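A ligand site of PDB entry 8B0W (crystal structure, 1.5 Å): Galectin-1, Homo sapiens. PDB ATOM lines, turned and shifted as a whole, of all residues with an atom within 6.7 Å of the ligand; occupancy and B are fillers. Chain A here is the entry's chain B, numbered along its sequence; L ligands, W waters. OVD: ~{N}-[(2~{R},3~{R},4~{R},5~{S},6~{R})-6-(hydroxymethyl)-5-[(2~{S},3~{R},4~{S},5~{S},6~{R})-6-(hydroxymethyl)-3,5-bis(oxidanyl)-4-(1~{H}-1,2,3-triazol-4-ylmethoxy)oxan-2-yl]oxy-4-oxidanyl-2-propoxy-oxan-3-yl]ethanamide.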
ATOM      1  N   SER A  28      -1.679  10.217  -0.610  1.00  0.00           N
ATOM      2  CA  SER A  28      -0.789  11.205  -0.025  1.00  0.00           C
ATOM      3  C   SER A  28      -0.567  12.265  -1.093  1.00  0.00           C
ATOM      4  O   SER A  28      -0.597  11.964  -2.279  1.00  0.00           O
ATOM      5  CB  SER A  28       0.531  10.555   0.428  1.00  0.00           C
ATOM      6  OG  SER A  28       1.642  11.422   0.459  1.00  0.00           O
ATOM      7  N   VAL A  30       1.677  16.293  -1.564  1.00  0.00           N
ATOM      8  CA  VAL A  30       2.713  17.153  -1.008  1.00  0.00           C
ATOM      9  C   VAL A  30       2.685  18.506  -1.674  1.00  0.00           C
ATOM     10  O   VAL A  30       2.563  18.595  -2.912  1.00  0.00           O
ATOM     11  CB  VAL A  30       4.123  16.534  -1.190  1.00  0.00           C
ATOM     12  CG1 VAL A  30       5.204  17.529  -0.871  1.00  0.00           C
ATOM     13  CG2 VAL A  30       4.282  15.291  -0.326  1.00  0.00           C
ATOM     14  N   ASN A  32       5.439  21.592  -1.311  1.00  0.00           N
ATOM     15  CA  ASN A  32       6.681  22.097  -0.756  1.00  0.00           C
ATOM     16  C   ASN A  32       6.807  23.577  -1.075  1.00  0.00           C
ATOM     17  O   ASN A  32       6.558  24.009  -2.210  1.00  0.00           O
ATOM     18  CB  ASN A  32       7.891  21.365  -1.333  1.00  0.00           C
ATOM     19  CG  ASN A  32       7.973  19.955  -0.859  1.00  0.00           C
ATOM     20  OD1 ASN A  32       7.512  19.641   0.255  1.00  0.00           O
ATOM     21  ND2 ASN A  32       8.631  19.077  -1.646  1.00  0.00           N
ATOM     22  N   HIS A  43       7.256  21.691   4.137  1.00  0.00           N
ATOM     23  CA  HIS A  43       6.852  20.460   3.481  1.00  0.00           C
ATOM     24  C   HIS A  43       5.490  20.080   4.049  1.00  0.00           C
ATOM     25  O   HIS A  43       5.397  19.697   5.218  1.00  0.00           O
ATOM     26  CB  HIS A  43       7.913  19.384   3.720  1.00  0.00           C
ATOM     27  CG  HIS A  43       7.506  18.004   3.315  1.00  0.00           C
ATOM     28  ND1 HIS A  43       7.487  17.593   2.004  1.00  0.00           N
ATOM     29  CD2 HIS A  43       7.221  16.895   4.057  1.00  0.00           C
ATOM     30  CE1 HIS A  43       7.124  16.320   1.941  1.00  0.00           C
ATOM     31  NE2 HIS A  43       6.966  15.880   3.175  1.00  0.00           N
ATOM     32  N   ASN A  45       2.292  17.746   3.917  1.00  0.00           N
ATOM     33  CA  ASN A  45       2.029  16.395   3.411  1.00  0.00           C
ATOM     34  C   ASN A  45       0.807  15.762   4.058  1.00  0.00           C
ATOM     35  O   ASN A  45       0.927  14.993   5.014  1.00  0.00           O
ATOM     36  CB  ASN A  45       3.309  15.564   3.598  1.00  0.00           C
ATOM     37  CG  ASN A  45       3.196  14.131   3.116  1.00  0.00           C
ATOM     38  OD1 ASN A  45       3.957  13.294   3.581  1.00  0.00           O
ATOM     39  ND2 ASN A  45       2.264  13.832   2.226  1.00  0.00           N
ATOM     40  N   ARG A  47      -1.590  12.938   4.512  1.00  0.00           N
ATOM     41  CA  ARG A  47      -1.474  11.507   4.275  1.00  0.00           C
ATOM     42  C   ARG A  47      -2.836  10.883   4.548  1.00  0.00           C
ATOM     43  O   ARG A  47      -3.300  10.871   5.687  1.00  0.00           O
ATOM     44  CB  ARG A  47      -0.397  10.895   5.159  1.00  0.00           C
ATOM     45  CG  ARG A  47       1.012  11.416   4.839  1.00  0.00           C
ATOM     46  CD  ARG A  47       2.013  10.973   5.845  1.00  0.00           C
ATOM     47  NE  ARG A  47       3.357  11.407   5.477  1.00  0.00           N
ATOM     48  CZ  ARG A  47       4.461  11.160   6.161  1.00  0.00           C
ATOM     49  NH1 ARG A  47       4.452  10.369   7.233  1.00  0.00           N
ATOM     50  NH2 ARG A  47       5.607  11.693   5.768  1.00  0.00           N
ATOM     51  N   ALA A  50      -0.519   6.551   4.210  1.00  0.00           N
ATOM     52  CA  ALA A  50       0.832   6.540   3.665  1.00  0.00           C
ATOM     53  C   ALA A  50       1.857   6.727   4.776  1.00  0.00           C
ATOM     54  O   ALA A  50       1.612   7.456   5.746  1.00  0.00           O
ATOM     55  CB  ALA A  50       1.008   7.629   2.601  1.00  0.00           C
ATOM     56  N   HIS A  51       2.996   6.065   4.595  1.00  0.00           N
ATOM     57  CA  HIS A  51       4.162   6.173   5.479  1.00  0.00           C
ATOM     58  C   HIS A  51       3.768   5.991   6.924  1.00  0.00           C
ATOM     59  O   HIS A  51       4.302   6.648   7.823  1.00  0.00           O
ATOM     60  CB  HIS A  51       4.895   7.501   5.280  1.00  0.00           C
ATOM     61  CG  HIS A  51       5.146   7.844   3.858  1.00  0.00           C
ATOM     62  ND1 HIS A  51       6.196   7.308   3.144  1.00  0.00           N
ATOM     63  CD2 HIS A  51       4.509   8.690   3.008  1.00  0.00           C
ATOM     64  CE1 HIS A  51       6.187   7.789   1.913  1.00  0.00           C
ATOM     65  NE2 HIS A  51       5.166   8.628   1.807  1.00  0.00           N
ATOM     66  N   GLY A  52       2.822   5.099   7.172  1.00  0.00           N
ATOM     67  CA  GLY A  52       2.458   4.769   8.516  1.00  0.00           C
ATOM     68  C   GLY A  52       1.466   5.692   9.182  1.00  0.00           C
ATOM     69  O   GLY A  52       1.271   5.602  10.397  1.00  0.00           O
ATOM     70  N   ASP A  53       0.814   6.577   8.427  1.00  0.00           N
ATOM     71  CA  ASP A  53      -0.137   7.540   8.934  1.00  0.00           C
ATOM     72  C   ASP A  53      -1.478   7.407   8.208  1.00  0.00           C
ATOM     73  O   ASP A  53      -1.521   7.248   6.988  1.00  0.00           O
ATOM     74  CB  ASP A  53       0.369   8.978   8.692  1.00  0.00           C
ATOM     75  CG  ASP A  53       1.446   9.397   9.664  1.00  0.00           C
ATOM     76  OD1 ASP A  53       1.148   9.534  10.864  1.00  0.00           O
ATOM     77  OD2 ASP A  53       2.585   9.618   9.219  1.00  0.00           O
ATOM     78  N   VAL A  58       1.230  15.721   7.948  1.00  0.00           N
ATOM     79  CA  VAL A  58       2.609  15.778   8.407  1.00  0.00           C
ATOM     80  C   VAL A  58       3.251  17.019   7.800  1.00  0.00           C
ATOM     81  O   VAL A  58       3.203  17.232   6.571  1.00  0.00           O
ATOM     82  CB  VAL A  58       3.384  14.511   8.034  1.00  0.00           C
ATOM     83  CG1 VAL A  58       4.839  14.634   8.455  1.00  0.00           C
ATOM     84  CG2 VAL A  58       2.743  13.303   8.690  1.00  0.00           C
ATOM     85  N   CYS A  59       3.850  17.844   8.630  1.00  0.00           N
ATOM     86  CA  CYS A  59       4.631  18.985   8.181  1.00  0.00           C
ATOM     87  C   CYS A  59       6.080  18.826   8.608  1.00  0.00           C
ATOM     88  O   CYS A  59       6.379  18.229   9.656  1.00  0.00           O
ATOM     89  CB  CYS A  59       4.105  20.279   8.755  1.00  0.00           C
ATOM     90  SG  CYS A  59       2.481  20.743   8.109  1.00  0.00           S
ATOM     91  N   ASN A  60       6.981  19.353   7.804  1.00  0.00           N
ATOM     92  CA  ASN A  60       8.396  19.391   8.133  1.00  0.00           C
ATOM     93  C   ASN A  60       9.059  20.545   7.398  1.00  0.00           C
ATOM     94  O   ASN A  60       8.443  21.236   6.589  1.00  0.00           O
ATOM     95  CB  ASN A  60       9.049  18.033   7.800  1.00  0.00           C
ATOM     96  CG  ASN A  60      10.247  17.727   8.652  1.00  0.00           C
ATOM     97  OD1 ASN A  60      10.753  18.595   9.351  1.00  0.00           O
ATOM     98  ND2 ASN A  60      10.724  16.480   8.594  1.00  0.00           N
ATOM     99  N   SER A  61      10.325  20.768   7.717  1.00  0.00           N
ATOM    100  CA  SER A  61      11.236  21.678   7.051  1.00  0.00           C
ATOM    101  C   SER A  61      12.394  20.875   6.477  1.00  0.00           C
ATOM    102  O   SER A  61      12.603  19.714   6.817  1.00  0.00           O
ATOM    103  CB  SER A  61      11.752  22.705   8.040  1.00  0.00           C
ATOM    104  OG  SER A  61      12.354  22.028   9.141  1.00  0.00           O
ATOM    105  N   TRP A  67      16.322  17.021   6.462  1.00  0.00           N
ATOM    106  CA  TRP A  67      14.972  17.107   6.996  1.00  0.00           C
ATOM    107  C   TRP A  67      15.031  17.509   8.456  1.00  0.00           C
ATOM    108  O   TRP A  67      15.889  17.058   9.233  1.00  0.00           O
ATOM    109  CB  TRP A  67      14.239  15.771   6.896  1.00  0.00           C
ATOM    110  CG  TRP A  67      13.805  15.387   5.535  1.00  0.00           C
ATOM    111  CD1 TRP A  67      14.283  14.354   4.794  1.00  0.00           C
ATOM    112  CD2 TRP A  67      12.758  15.988   4.754  1.00  0.00           C
ATOM    113  NE1 TRP A  67      13.637  14.287   3.592  1.00  0.00           N
ATOM    114  CE2 TRP A  67      12.682  15.277   3.541  1.00  0.00           C
ATOM    115  CE3 TRP A  67      11.884  17.052   4.952  1.00  0.00           C
ATOM    116  CZ2 TRP A  67      11.782  15.613   2.528  1.00  0.00           C
ATOM    117  CZ3 TRP A  67      10.992  17.381   3.969  1.00  0.00           C
ATOM    118  CH2 TRP A  67      10.947  16.679   2.759  1.00  0.00           C
ATOM    119  N   GLY A  68      14.067  18.334   8.857  1.00  0.00           N
ATOM    120  CA  GLY A  68      13.844  18.650  10.244  1.00  0.00           C
ATOM    121  C   GLY A  68      13.006  17.598  10.954  1.00  0.00           C
ATOM    122  O   GLY A  68      12.854  16.453  10.524  1.00  0.00           O
ATOM    123  N   THR A  69      12.445  18.042  12.070  1.00  0.00           N
ATOM    124  CA  THR A  69      11.603  17.214  12.913  1.00  0.00           C
ATOM    125  C   THR A  69      10.163  17.358  12.446  1.00  0.00           C
ATOM    126  O   THR A  69       9.671  18.491  12.344  1.00  0.00           O
ATOM    127  CB  THR A  69      11.749  17.614  14.379  1.00  0.00           C
ATOM    128  OG1 THR A  69      13.097  17.330  14.808  1.00  0.00           O
ATOM    129  CG2 THR A  69      10.754  16.872  15.244  1.00  0.00           C
ATOM    130  N   GLU A  70       9.494  16.240  12.200  1.00  0.00           N
ATOM    131  CA  GLU A  70       8.114  16.266  11.766  1.00  0.00           C
ATOM    132  C   GLU A  70       7.202  16.835  12.851  1.00  0.00           C
ATOM    133  O   GLU A  70       7.395  16.601  14.055  1.00  0.00           O
ATOM    134  CB  GLU A  70       7.631  14.860  11.429  1.00  0.00           C
ATOM    135  CG  GLU A  70       8.198  14.318  10.127  1.00  0.00           C
ATOM    136  CD  GLU A  70       7.900  12.841   9.883  1.00  0.00           C
ATOM    137  OE1 GLU A  70       7.356  12.148  10.754  1.00  0.00           O
ATOM    138  OE2 GLU A  70       8.251  12.370   8.784  1.00  0.00           O
ATOM    139  N   ARG A  72       2.921  16.776  13.455  1.00  0.00           N
ATOM    140  CA  ARG A  72       1.659  16.230  12.981  1.00  0.00           C
ATOM    141  C   ARG A  72       0.505  17.083  13.457  1.00  0.00           C
ATOM    142  O   ARG A  72       0.434  17.438  14.647  1.00  0.00           O
ATOM    143  CB  ARG A  72       1.463  14.776  13.445  1.00  0.00           C
ATOM    144  CG  ARG A  72       2.199  13.820  12.522  1.00  0.00           C
ATOM    145  CD  ARG A  72       2.228  12.392  13.056  1.00  0.00           C
ATOM    146  NE  ARG A  72       2.892  11.524  12.086  1.00  0.00           N
ATOM    147  CZ  ARG A  72       4.190  11.573  11.812  1.00  0.00           C
ATOM    148  NH1 ARG A  72       5.008  12.416  12.434  1.00  0.00           N
ATOM    149  NH2 ARG A  72       4.686  10.767  10.887  1.00  0.00           N
ATOM    150  N   ASP A 122       3.647  17.340  -5.449  1.00  0.00           N
ATOM    151  CA  ASP A 122       3.919  15.941  -5.743  1.00  0.00           C
ATOM    152  C   ASP A 122       2.751  15.131  -5.210  1.00  0.00           C
ATOM    153  O   ASP A 122       1.990  15.589  -4.354  1.00  0.00           O
ATOM    154  CB  ASP A 122       5.249  15.484  -5.127  1.00  0.00           C
ATOM    155  CG  ASP A 122       6.420  16.411  -5.466  1.00  0.00           C
ATOM    156  OD1 ASP A 122       6.826  17.211  -4.597  1.00  0.00           O
ATOM    157  OD2 ASP A 122       6.931  16.340  -6.611  1.00  0.00           O
ATOM    158  N   GLY A 123       2.605  13.924  -5.732  1.00  0.00           N
ATOM    159  CA  GLY A 123       1.605  13.031  -5.198  1.00  0.00           C
ATOM    160  C   GLY A 123       0.227  13.240  -5.780  1.00  0.00           C
ATOM    161  O   GLY A 123       0.082  13.702  -6.917  1.00  0.00           O
HETATM  162  C4  OVD L   1       8.843   9.200   6.998  1.00  0.00           C
HETATM  163  C5  OVD L   1       9.573   7.885   6.824  1.00  0.00           C
HETATM  164  C6  OVD L   1      10.835   8.043   5.996  1.00  0.00           C
HETATM  165  C7  OVD L   1       6.436   7.975  11.114  1.00  0.00           C
HETATM  166  C8  OVD L   1       5.034   7.539  11.559  1.00  0.00           C
HETATM  167  N2  OVD L   1       6.636   7.962   9.775  1.00  0.00           N
HETATM  168  C3  OVD L   1       7.623   8.954   7.850  1.00  0.00           C
HETATM  169  C1  OVD L   1       8.779   7.025   8.801  1.00  0.00           C
HETATM  170  C2  OVD L   1       7.949   8.270   9.156  1.00  0.00           C
HETATM  171  CAF OVD L   1       8.897   4.831  10.031  1.00  0.00           C
HETATM  172  CAM OVD L   1       7.414   5.113   9.781  1.00  0.00           C
HETATM  173  CAO OVD L   1       8.977  14.359   5.845  1.00  0.00           C
HETATM  174  CAP OVD L   1       8.532  10.699   3.624  1.00  0.00           C
HETATM  175  CAQ OVD L   1       9.102  11.894   2.900  1.00  0.00           C
HETATM  176  CAR OVD L   1       8.733  13.154   3.672  1.00  0.00           C
HETATM  177  CAS OVD L   1       9.282  13.048   5.074  1.00  0.00           C
HETATM  178  CAU OVD L   1       9.063  10.669   5.038  1.00  0.00           C
HETATM  179  CAY OVD L   1       6.558   4.396   8.800  1.00  0.00           C
HETATM  180  CAZ OVD L   1       9.339  12.694   0.696  1.00  0.00           C
HETATM  181  CBA OVD L   1       8.539  12.877  -0.576  1.00  0.00           C
HETATM  182  CBB OVD L   1       8.392  11.968  -1.524  1.00  0.00           C
HETATM  183  NBC OVD L   1       7.613  12.570  -2.423  1.00  0.00           N
HETATM  184  NBD OVD L   1       7.322  13.734  -2.014  1.00  0.00           N
HETATM  185  NBE OVD L   1       7.857  13.965  -0.910  1.00  0.00           N
HETATM  186  O1  OVD L   1       9.206   6.256   9.999  1.00  0.00           O
HETATM  187  O3  OVD L   1       6.952  10.230   8.180  1.00  0.00           O
HETATM  188  O4  OVD L   1       8.423   9.582   5.703  1.00  0.00           O
HETATM  189  O5  OVD L   1       9.955   7.385   8.099  1.00  0.00           O
HETATM  190  O6  OVD L   1      11.753   8.887   6.703  1.00  0.00           O
HETATM  191  O7  OVD L   1       7.285   8.297  11.929  1.00  0.00           O
HETATM  192  OAN OVD L   1       8.915   9.464   2.971  1.00  0.00           O
HETATM  193  OAT OVD L   1       8.702  11.884   5.713  1.00  0.00           O
HETATM  194  OAV OVD L   1       7.292  13.240   3.672  1.00  0.00           O
HETATM  195  OAW OVD L   1       9.426  14.194   7.169  1.00  0.00           O
HETATM  196  OAX OVD L   1       8.514  11.957   1.611  1.00  0.00           O
HETATM  197  O   HOH W   1       5.605  12.191   1.466  1.00  0.00           O
HETATM  198  O   HOH W   2       9.391  16.260  -0.695  1.00  0.00           O
HETATM  199  O   HOH W   3       9.287  11.096  12.124  1.00  0.00           O
HETATM  200  O   HOH W   4      10.284   8.433  11.679  1.00  0.00           O
HETATM  201  O   HOH W   5      11.806  13.078   7.881  1.00  0.00           O
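NE2 of His 43 lies within hydrogen-bond range of OAV of the ligand (2.7 Å). NH1 of Arg 47 lies within hydrogen-bond range of O3 of the ligand (2.7 Å). The side-chain amide oxygen (OD1) of Asn 45 lies within hydrogen-bond range of an oxygen (OAV) of the ligand (3.3 Å). ND2 of Asn 60 lies within hydrogen-bond range of OAW of the ligand, 3.0 Å away. OE2 of Glu 70 lies within hydrogen-bond range of O3 of the ligand (2.6 Å). The backbone carbonyl oxygen of His 51 sits at hydrogen-bond distance from a nitrogen (N2) of the ligand (3.3 Å). A ring nitrogen (ND1) of His 51 sits close to an oxygen (OAN) of the ligand, at 3.5 Å.
OD1 of Asp 53 is in salt-bridge range of NE of Arg 72, 2.9 Å away. The side-chain amide oxygen (OD1) of Asn 32 sits at hydrogen-bond distance from a ring nitrogen (ND1) of His 43 (2.7 Å). N of Asn 45 sits at hydrogen-bond distance from O of Val 58 (2.9 Å). NH1 of Arg 47 is in salt-bridge range of OD2 of Asp 53 (2.8 Å). N of Val 30 sits at hydrogen-bond distance from O of Asp 122 (2.9 Å). The backbone carbonyl oxygen of Asn 60 is in hydrogen-bond range of the backbone NH of His 43. The side-chain hydroxyl of Ser 28 is in hydrogen-bond range of the side-chain amide nitrogen of Asn 45 (3.1 Å). The side-chain carboxylate (OE1) of Glu 70 lies within salt-bridge range of the guanidinium group (NH1) of Arg 72.
Val 30 touches the ligand. OD2 of Asp 53 touches C8 of the ligand, 3.97 Å away. Arg 72 touches the ligand. Hydrophobic or aromatic side chains that line the ligand: Val 30, His 43 and His 51. Nine residues have an atom within 4 Å of the ligand: Val 30, His 43, Asn 45, Arg 47, His 51, Asp 53, Asn 60, Glu 70 and Arg 72.
Water W2 lies within hydrogen-bond range of a nitrogen (NBE) of the ligand (2.8 Å) and the side-chain amide nitrogen of Asn 32 (3.1 Å). Water W1 lies within hydrogen-bond range of the side-chain amide oxygen of Asn 45 (2.9 Å) and an oxygen (OAX) of the ligand (2.9 Å). Water W3 bridges the side-chain carboxylate of Glu 70 and an oxygen (O7) of the ligand.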
